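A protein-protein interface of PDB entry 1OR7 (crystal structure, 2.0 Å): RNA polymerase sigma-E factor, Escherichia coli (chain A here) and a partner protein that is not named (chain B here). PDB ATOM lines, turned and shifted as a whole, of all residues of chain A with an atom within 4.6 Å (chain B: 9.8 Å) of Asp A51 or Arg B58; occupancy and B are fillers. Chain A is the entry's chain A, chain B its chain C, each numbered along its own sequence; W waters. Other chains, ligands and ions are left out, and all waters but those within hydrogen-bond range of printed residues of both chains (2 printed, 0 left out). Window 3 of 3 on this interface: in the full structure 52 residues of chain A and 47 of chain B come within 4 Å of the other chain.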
ATOM      1  N   ASP A  48      19.104  28.592   2.912  1.00  0.00           N
ATOM      2  CA  ASP A  48      20.032  27.500   2.708  1.00  0.00           C
ATOM      3  C   ASP A  48      20.171  27.111   1.272  1.00  0.00           C
ATOM      4  O   ASP A  48      21.006  26.276   0.944  1.00  0.00           O
ATOM      5  CB  ASP A  48      19.595  26.281   3.484  1.00  0.00           C
ATOM      6  CG  ASP A  48      19.632  26.505   4.953  1.00  0.00           C
ATOM      7  OD1 ASP A  48      20.647  27.025   5.464  1.00  0.00           O
ATOM      8  OD2 ASP A  48      18.681  26.184   5.680  1.00  0.00           O
ATOM      9  N   VAL A  49      19.362  27.714   0.423  1.00  0.00           N
ATOM     10  CA  VAL A  49      19.351  27.354  -0.992  1.00  0.00           C
ATOM     11  C   VAL A  49      20.725  27.443  -1.700  1.00  0.00           C
ATOM     12  O   VAL A  49      21.104  26.519  -2.417  1.00  0.00           O
ATOM     13  CB  VAL A  49      18.307  28.167  -1.741  1.00  0.00           C
ATOM     14  CG1 VAL A  49      18.460  27.992  -3.229  1.00  0.00           C
ATOM     15  CG2 VAL A  49      16.910  27.737  -1.315  1.00  0.00           C
ATOM     16  N   PRO A  50      21.475  28.522  -1.528  1.00  0.00           N
ATOM     17  CA  PRO A  50      22.783  28.611  -2.186  1.00  0.00           C
ATOM     18  C   PRO A  50      23.728  27.490  -1.777  1.00  0.00           C
ATOM     19  O   PRO A  50      24.350  26.884  -2.639  1.00  0.00           O
ATOM     20  CB  PRO A  50      23.326  29.973  -1.741  1.00  0.00           C
ATOM     21  CG  PRO A  50      22.098  30.750  -1.391  1.00  0.00           C
ATOM     22  CD  PRO A  50      21.172  29.732  -0.750  1.00  0.00           C
ATOM     23  N   ASP A  51      23.813  27.198  -0.487  1.00  0.00           N
ATOM     24  CA  ASP A  51      24.699  26.141  -0.014  1.00  0.00           C
ATOM     25  C   ASP A  51      24.308  24.768  -0.560  1.00  0.00           C
ATOM     26  O   ASP A  51      25.166  23.962  -0.903  1.00  0.00           O
ATOM     27  CB  ASP A  51      24.710  26.074   1.504  1.00  0.00           C
ATOM     28  CG  ASP A  51      25.502  27.193   2.155  1.00  0.00           C
ATOM     29  OD1 ASP A  51      26.302  27.898   1.485  1.00  0.00           O
ATOM     30  OD2 ASP A  51      25.391  27.419   3.378  1.00  0.00           O
ATOM     31  N   VAL A  52      23.018  24.481  -0.582  1.00  0.00           N
ATOM     32  CA  VAL A  52      22.537  23.204  -1.097  1.00  0.00           C
ATOM     33  C   VAL A  52      22.794  23.112  -2.611  1.00  0.00           C
ATOM     34  O   VAL A  52      23.281  22.100  -3.092  1.00  0.00           O
ATOM     35  CB  VAL A  52      21.036  22.971  -0.732  1.00  0.00           C
ATOM     36  CG1 VAL A  52      20.480  21.741  -1.387  1.00  0.00           C
ATOM     37  CG2 VAL A  52      20.879  22.815   0.758  1.00  0.00           C
ATOM     38  N   VAL A  53      22.490  24.175  -3.353  1.00  0.00           N
ATOM     39  CA  VAL A  53      22.746  24.201  -4.790  1.00  0.00           C
ATOM     40  C   VAL A  53      24.239  23.944  -5.056  1.00  0.00           C
ATOM     41  O   VAL A  53      24.616  23.163  -5.936  1.00  0.00           O
ATOM     42  CB  VAL A  53      22.323  25.554  -5.401  1.00  0.00           C
ATOM     43  CG1 VAL A  53      22.856  25.678  -6.847  1.00  0.00           C
ATOM     44  CG2 VAL A  53      20.801  25.680  -5.411  1.00  0.00           C
ATOM     45  N   GLN A  54      25.078  24.595  -4.271  1.00  0.00           N
ATOM     46  CA  GLN A  54      26.523  24.443  -4.383  1.00  0.00           C
ATOM     47  C   GLN A  54      26.932  22.993  -4.168  1.00  0.00           C
ATOM     48  O   GLN A  54      27.639  22.412  -4.978  1.00  0.00           O
ATOM     49  CB  GLN A  54      27.211  25.310  -3.331  1.00  0.00           C
ATOM     50  CG  GLN A  54      28.726  25.101  -3.246  1.00  0.00           C
ATOM     51  CD  GLN A  54      29.453  26.139  -4.042  1.00  0.00           C
ATOM     52  OE1 GLN A  54      29.020  27.283  -4.078  1.00  0.00           O
ATOM     53  NE2 GLN A  54      30.567  25.763  -4.667  1.00  0.00           N
ATOM     54  N   GLU A  55      26.471  22.414  -3.068  1.00  0.00           N
ATOM     55  CA  GLU A  55      26.764  21.026  -2.756  1.00  0.00           C
ATOM     56  C   GLU A  55      26.224  20.094  -3.853  1.00  0.00           C
ATOM     57  O   GLU A  55      26.844  19.088  -4.173  1.00  0.00           O
ATOM     58  CB  GLU A  55      26.193  20.651  -1.373  1.00  0.00           C
ATOM     59  CG  GLU A  55      26.558  19.241  -0.930  1.00  0.00           C
ATOM     60  CD  GLU A  55      26.019  18.867   0.447  1.00  0.00           C
ATOM     61  OE1 GLU A  55      25.826  19.776   1.310  1.00  0.00           O
ATOM     62  OE2 GLU A  55      25.785  17.649   0.675  1.00  0.00           O
ATOM     63  N   GLU B  34      25.453  33.197 -20.611  1.00  0.00           N
ATOM     64  CA  GLU B  34      24.795  33.398 -19.325  1.00  0.00           C
ATOM     65  C   GLU B  34      23.489  34.161 -19.504  1.00  0.00           C
ATOM     66  O   GLU B  34      22.439  33.728 -19.002  1.00  0.00           O
ATOM     67  CB  GLU B  34      25.759  34.140 -18.386  1.00  0.00           C
ATOM     68  CG  GLU B  34      25.196  34.587 -17.060  1.00  0.00           C
ATOM     69  CD  GLU B  34      26.243  35.321 -16.224  1.00  0.00           C
ATOM     70  OE1 GLU B  34      26.523  36.486 -16.503  1.00  0.00           O
ATOM     71  OE2 GLU B  34      26.813  34.718 -15.295  1.00  0.00           O
ATOM     72  N   HIS B  52      19.840  34.295  -7.653  1.00  0.00           N
ATOM     73  CA  HIS B  52      21.158  34.613  -7.182  1.00  0.00           C
ATOM     74  C   HIS B  52      22.077  34.574  -8.388  1.00  0.00           C
ATOM     75  O   HIS B  52      22.047  33.630  -9.158  1.00  0.00           O
ATOM     76  CB  HIS B  52      21.585  33.564  -6.181  1.00  0.00           C
ATOM     77  CG  HIS B  52      20.855  33.653  -4.884  1.00  0.00           C
ATOM     78  ND1 HIS B  52      21.446  34.126  -3.733  1.00  0.00           N
ATOM     79  CD2 HIS B  52      19.584  33.342  -4.554  1.00  0.00           C
ATOM     80  CE1 HIS B  52      20.569  34.110  -2.753  1.00  0.00           C
ATOM     81  NE2 HIS B  52      19.433  33.634  -3.222  1.00  0.00           N
ATOM     82  N   PHE B  53      22.911  35.575  -8.561  1.00  0.00           N
ATOM     83  CA  PHE B  53      23.753  35.617  -9.753  1.00  0.00           C
ATOM     84  C   PHE B  53      25.186  35.194  -9.506  1.00  0.00           C
ATOM     85  O   PHE B  53      26.025  35.346 -10.396  1.00  0.00           O
ATOM     86  CB  PHE B  53      23.760  37.030 -10.329  1.00  0.00           C
ATOM     87  CG  PHE B  53      22.445  37.467 -10.824  1.00  0.00           C
ATOM     88  CD1 PHE B  53      21.804  38.542 -10.267  1.00  0.00           C
ATOM     89  CD2 PHE B  53      21.847  36.803 -11.867  1.00  0.00           C
ATOM     90  CE1 PHE B  53      20.569  38.945 -10.735  1.00  0.00           C
ATOM     91  CE2 PHE B  53      20.637  37.182 -12.328  1.00  0.00           C
ATOM     92  CZ  PHE B  53      19.974  38.246 -11.762  1.00  0.00           C
ATOM     93  N   ASP B  54      25.484  34.679  -8.320  1.00  0.00           N
ATOM     94  CA  ASP B  54      26.831  34.234  -8.022  1.00  0.00           C
ATOM     95  C   ASP B  54      26.964  32.718  -7.938  1.00  0.00           C
ATOM     96  O   ASP B  54      27.969  32.211  -7.474  1.00  0.00           O
ATOM     97  CB  ASP B  54      27.288  34.831  -6.689  1.00  0.00           C
ATOM     98  CG  ASP B  54      26.480  34.317  -5.518  1.00  0.00           C
ATOM     99  OD1 ASP B  54      25.426  33.644  -5.727  1.00  0.00           O
ATOM    100  OD2 ASP B  54      26.826  34.523  -4.343  1.00  0.00           O
ATOM    101  N   ILE B  55      25.955  31.982  -8.362  1.00  0.00           N
ATOM    102  CA  ILE B  55      26.026  30.549  -8.213  1.00  0.00           C
ATOM    103  C   ILE B  55      27.210  29.925  -8.951  1.00  0.00           C
ATOM    104  O   ILE B  55      28.012  29.232  -8.352  1.00  0.00           O
ATOM    105  CB  ILE B  55      24.712  29.911  -8.658  1.00  0.00           C
ATOM    106  CG1 ILE B  55      23.559  30.382  -7.746  1.00  0.00           C
ATOM    107  CG2 ILE B  55      24.816  28.397  -8.609  1.00  0.00           C
ATOM    108  CD1 ILE B  55      22.166  29.944  -8.267  1.00  0.00           C
ATOM    109  N   SER B  56      27.339  30.176 -10.242  1.00  0.00           N
ATOM    110  CA  SER B  56      28.359  29.500 -11.014  1.00  0.00           C
ATOM    111  C   SER B  56      29.746  29.877 -10.539  1.00  0.00           C
ATOM    112  O   SER B  56      30.636  29.045 -10.518  1.00  0.00           O
ATOM    113  CB  SER B  56      28.179  29.762 -12.523  1.00  0.00           C
ATOM    114  OG  SER B  56      28.297  31.150 -12.834  1.00  0.00           O
ATOM    115  N   SER B  57      29.928  31.119 -10.113  1.00  0.00           N
ATOM    116  CA  SER B  57      31.254  31.547  -9.662  1.00  0.00           C
ATOM    117  C   SER B  57      31.616  30.816  -8.388  1.00  0.00           C
ATOM    118  O   SER B  57      32.742  30.343  -8.230  1.00  0.00           O
ATOM    119  CB  SER B  57      31.331  33.069  -9.459  1.00  0.00           C
ATOM    120  OG  SER B  57      30.291  33.529  -8.609  1.00  0.00           O
ATOM    121  N   ARG B  58      30.654  30.698  -7.485  1.00  0.00           N
ATOM    122  CA  ARG B  58      30.887  29.944  -6.258  1.00  0.00           C
ATOM    123  C   ARG B  58      31.198  28.474  -6.529  1.00  0.00           C
ATOM    124  O   ARG B  58      32.071  27.887  -5.883  1.00  0.00           O
ATOM    125  CB  ARG B  58      29.668  30.013  -5.347  1.00  0.00           C
ATOM    126  CG  ARG B  58      29.475  31.334  -4.644  1.00  0.00           C
ATOM    127  CD  ARG B  58      28.346  31.302  -3.612  1.00  0.00           C
ATOM    128  NE  ARG B  58      28.443  30.141  -2.713  1.00  0.00           N
ATOM    129  CZ  ARG B  58      27.497  29.783  -1.844  1.00  0.00           C
ATOM    130  NH1 ARG B  58      26.383  30.494  -1.744  1.00  0.00           N
ATOM    131  NH2 ARG B  58      27.668  28.726  -1.061  1.00  0.00           N
ATOM    132  N   VAL B  59      30.457  27.867  -7.451  1.00  0.00           N
ATOM    133  CA  VAL B  59      30.698  26.480  -7.802  1.00  0.00           C
ATOM    134  C   VAL B  59      32.106  26.302  -8.357  1.00  0.00           C
ATOM    135  O   VAL B  59      32.880  25.508  -7.852  1.00  0.00           O
ATOM    136  CB  VAL B  59      29.673  25.967  -8.834  1.00  0.00           C
ATOM    137  CG1 VAL B  59      30.093  24.629  -9.373  1.00  0.00           C
ATOM    138  CG2 VAL B  59      28.311  25.855  -8.198  1.00  0.00           C
ATOM    139  N   MET B  60      32.449  27.075  -9.375  1.00  0.00           N
ATOM    140  CA  MET B  60      33.757  26.944  -9.997  1.00  0.00           C
ATOM    141  C   MET B  60      34.901  27.198  -9.002  1.00  0.00           C
ATOM    142  O   MET B  60      35.941  26.548  -9.070  1.00  0.00           O
ATOM    143  CB  MET B  60      33.875  27.879 -11.200  1.00  0.00           C
ATOM    144  CG  MET B  60      32.904  27.554 -12.327  1.00  0.00           C
ATOM    145  SD  MET B  60      32.903  25.627 -12.726  1.00  0.00           S
ATOM    146  CE  MET B  60      34.852  25.504 -13.184  1.00  0.00           C
ATOM    147  N   ALA B  61      34.718  28.136  -8.079  1.00  0.00           N
ATOM    148  CA  ALA B  61      35.764  28.395  -7.098  1.00  0.00           C
ATOM    149  C   ALA B  61      35.970  27.142  -6.247  1.00  0.00           C
ATOM    150  O   ALA B  61      37.082  26.856  -5.821  1.00  0.00           O
ATOM    151  CB  ALA B  61      35.417  29.604  -6.228  1.00  0.00           C
ATOM    152  N   ALA B  62      34.903  26.388  -6.007  1.00  0.00           N
ATOM    153  CA  ALA B  62      35.009  25.153  -5.226  1.00  0.00           C
ATOM    154  C   ALA B  62      35.632  24.009  -6.044  1.00  0.00           C
ATOM    155  O   ALA B  62      36.270  23.106  -5.496  1.00  0.00           O
ATOM    156  CB  ALA B  62      33.655  24.754  -4.707  1.00  0.00           C
ATOM    157  N   ILE B  63      35.444  24.062  -7.355  1.00  0.00           N
ATOM    158  CA  ILE B  63      36.014  23.076  -8.251  1.00  0.00           C
ATOM    159  C   ILE B  63      37.519  23.286  -8.344  1.00  0.00           C
ATOM    160  O   ILE B  63      38.290  22.329  -8.344  1.00  0.00           O
ATOM    161  CB  ILE B  63      35.385  23.205  -9.657  1.00  0.00           C
ATOM    162  CG1 ILE B  63      33.893  22.884  -9.631  1.00  0.00           C
ATOM    163  CG2 ILE B  63      36.102  22.296 -10.651  1.00  0.00           C
ATOM    164  CD1 ILE B  63      33.567  21.487  -9.172  1.00  0.00           C
ATOM    165  N   GLU B  64      37.937  24.548  -8.407  1.00  0.00           N
ATOM    166  CA  GLU B  64      39.351  24.889  -8.537  1.00  0.00           C
ATOM    167  C   GLU B  64      40.211  24.346  -7.400  1.00  0.00           C
ATOM    168  O   GLU B  64      41.403  24.107  -7.586  1.00  0.00           O
ATOM    169  N   GLU B  65      39.599  24.153  -6.232  1.00  0.00           N
ATOM    170  CA  GLU B  65      40.289  23.662  -5.037  1.00  0.00           C
ATOM    171  C   GLU B  65      40.231  22.140  -4.892  1.00  0.00           C
ATOM    172  O   GLU B  65      40.754  21.582  -3.930  1.00  0.00           O
ATOM    173  CB  GLU B  65      39.679  24.299  -3.780  1.00  0.00           C
ATOM    174  CG  GLU B  65      40.034  25.766  -3.579  1.00  0.00           C
HETATM  175  O   HOH W   1      25.280  28.858  -4.473  1.00  0.00           O
HETATM  176  O   HOH W   2      27.169  28.099  -5.865  1.00  0.00           O
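The side-chain amide nitrogen (NE2) of Gln A54 lies close to the backbone NH (N) of Val B59 (3.5 Å). The side-chain carboxylate of Asp A51 is in salt-bridge range of the guanidinium group of Arg B58 (3.0 Å). The side-chain amide nitrogen (NE2) of Gln A54 lies within hydrogen-bond range of the backbone carbonyl oxygen (O) of Arg B58, at 2.9 Å.
Among the printed residues, merely in contact across the chains: Pro A50 with Arg B58, Gln A54 with Ala B62, Val A53 with Ile B55 and Pro A50 with His B52.
Water W2 lies within hydrogen-bond range of OE1 of Gln A54 (2.7 Å) and O of Ile B55 (2.9 Å). Water W1 bridges O of Pro A50 (2.9 Å) and NH1 of Arg B58 (3.4 Å).
Of chain A, only Pro A50, Asp A51 and Gln A54 come within 4 Å of Arg B58. Pro A50 touches just these residues of chain B: His B52 (3.9 Å) and Arg B58 (3.1 Å). No residue of chain B comes within 4 Å of Val A52. Of chain B, only Arg B58, Val B59 and Ala B62 come within 4 Å of Gln A54. Of the printed residues of chain A, His B52 touches Pro A50 (3.9 Å). Printed residues of chain A within 4 Å of Ala B62: Gln A54. Of the printed residues of chain A, Ile B55 touches Val A53. Glu B64 touches none of the printed residues of chain A. The nearest residue of chain B that does not touch Asp A51 is Ile B55 (7.9 Å). The nearest printed residue of chain A that does not touch Arg B58 is Val A52 (6.3 Å). The nearest printed residue of chain A that does not touch Ala B62 is Glu A55 (7.7 Å).
Hydrophobic or aromatic side chains of chain A within 4 Å of the printed part of chain B: Pro A50 and Val A53. Printed residues of chain B that touch a printed residue of chain A: His B52, Ile B55, Arg B58, Val B59 and Ala B62. Among the printed residues, 7 pairs touch across the chains.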
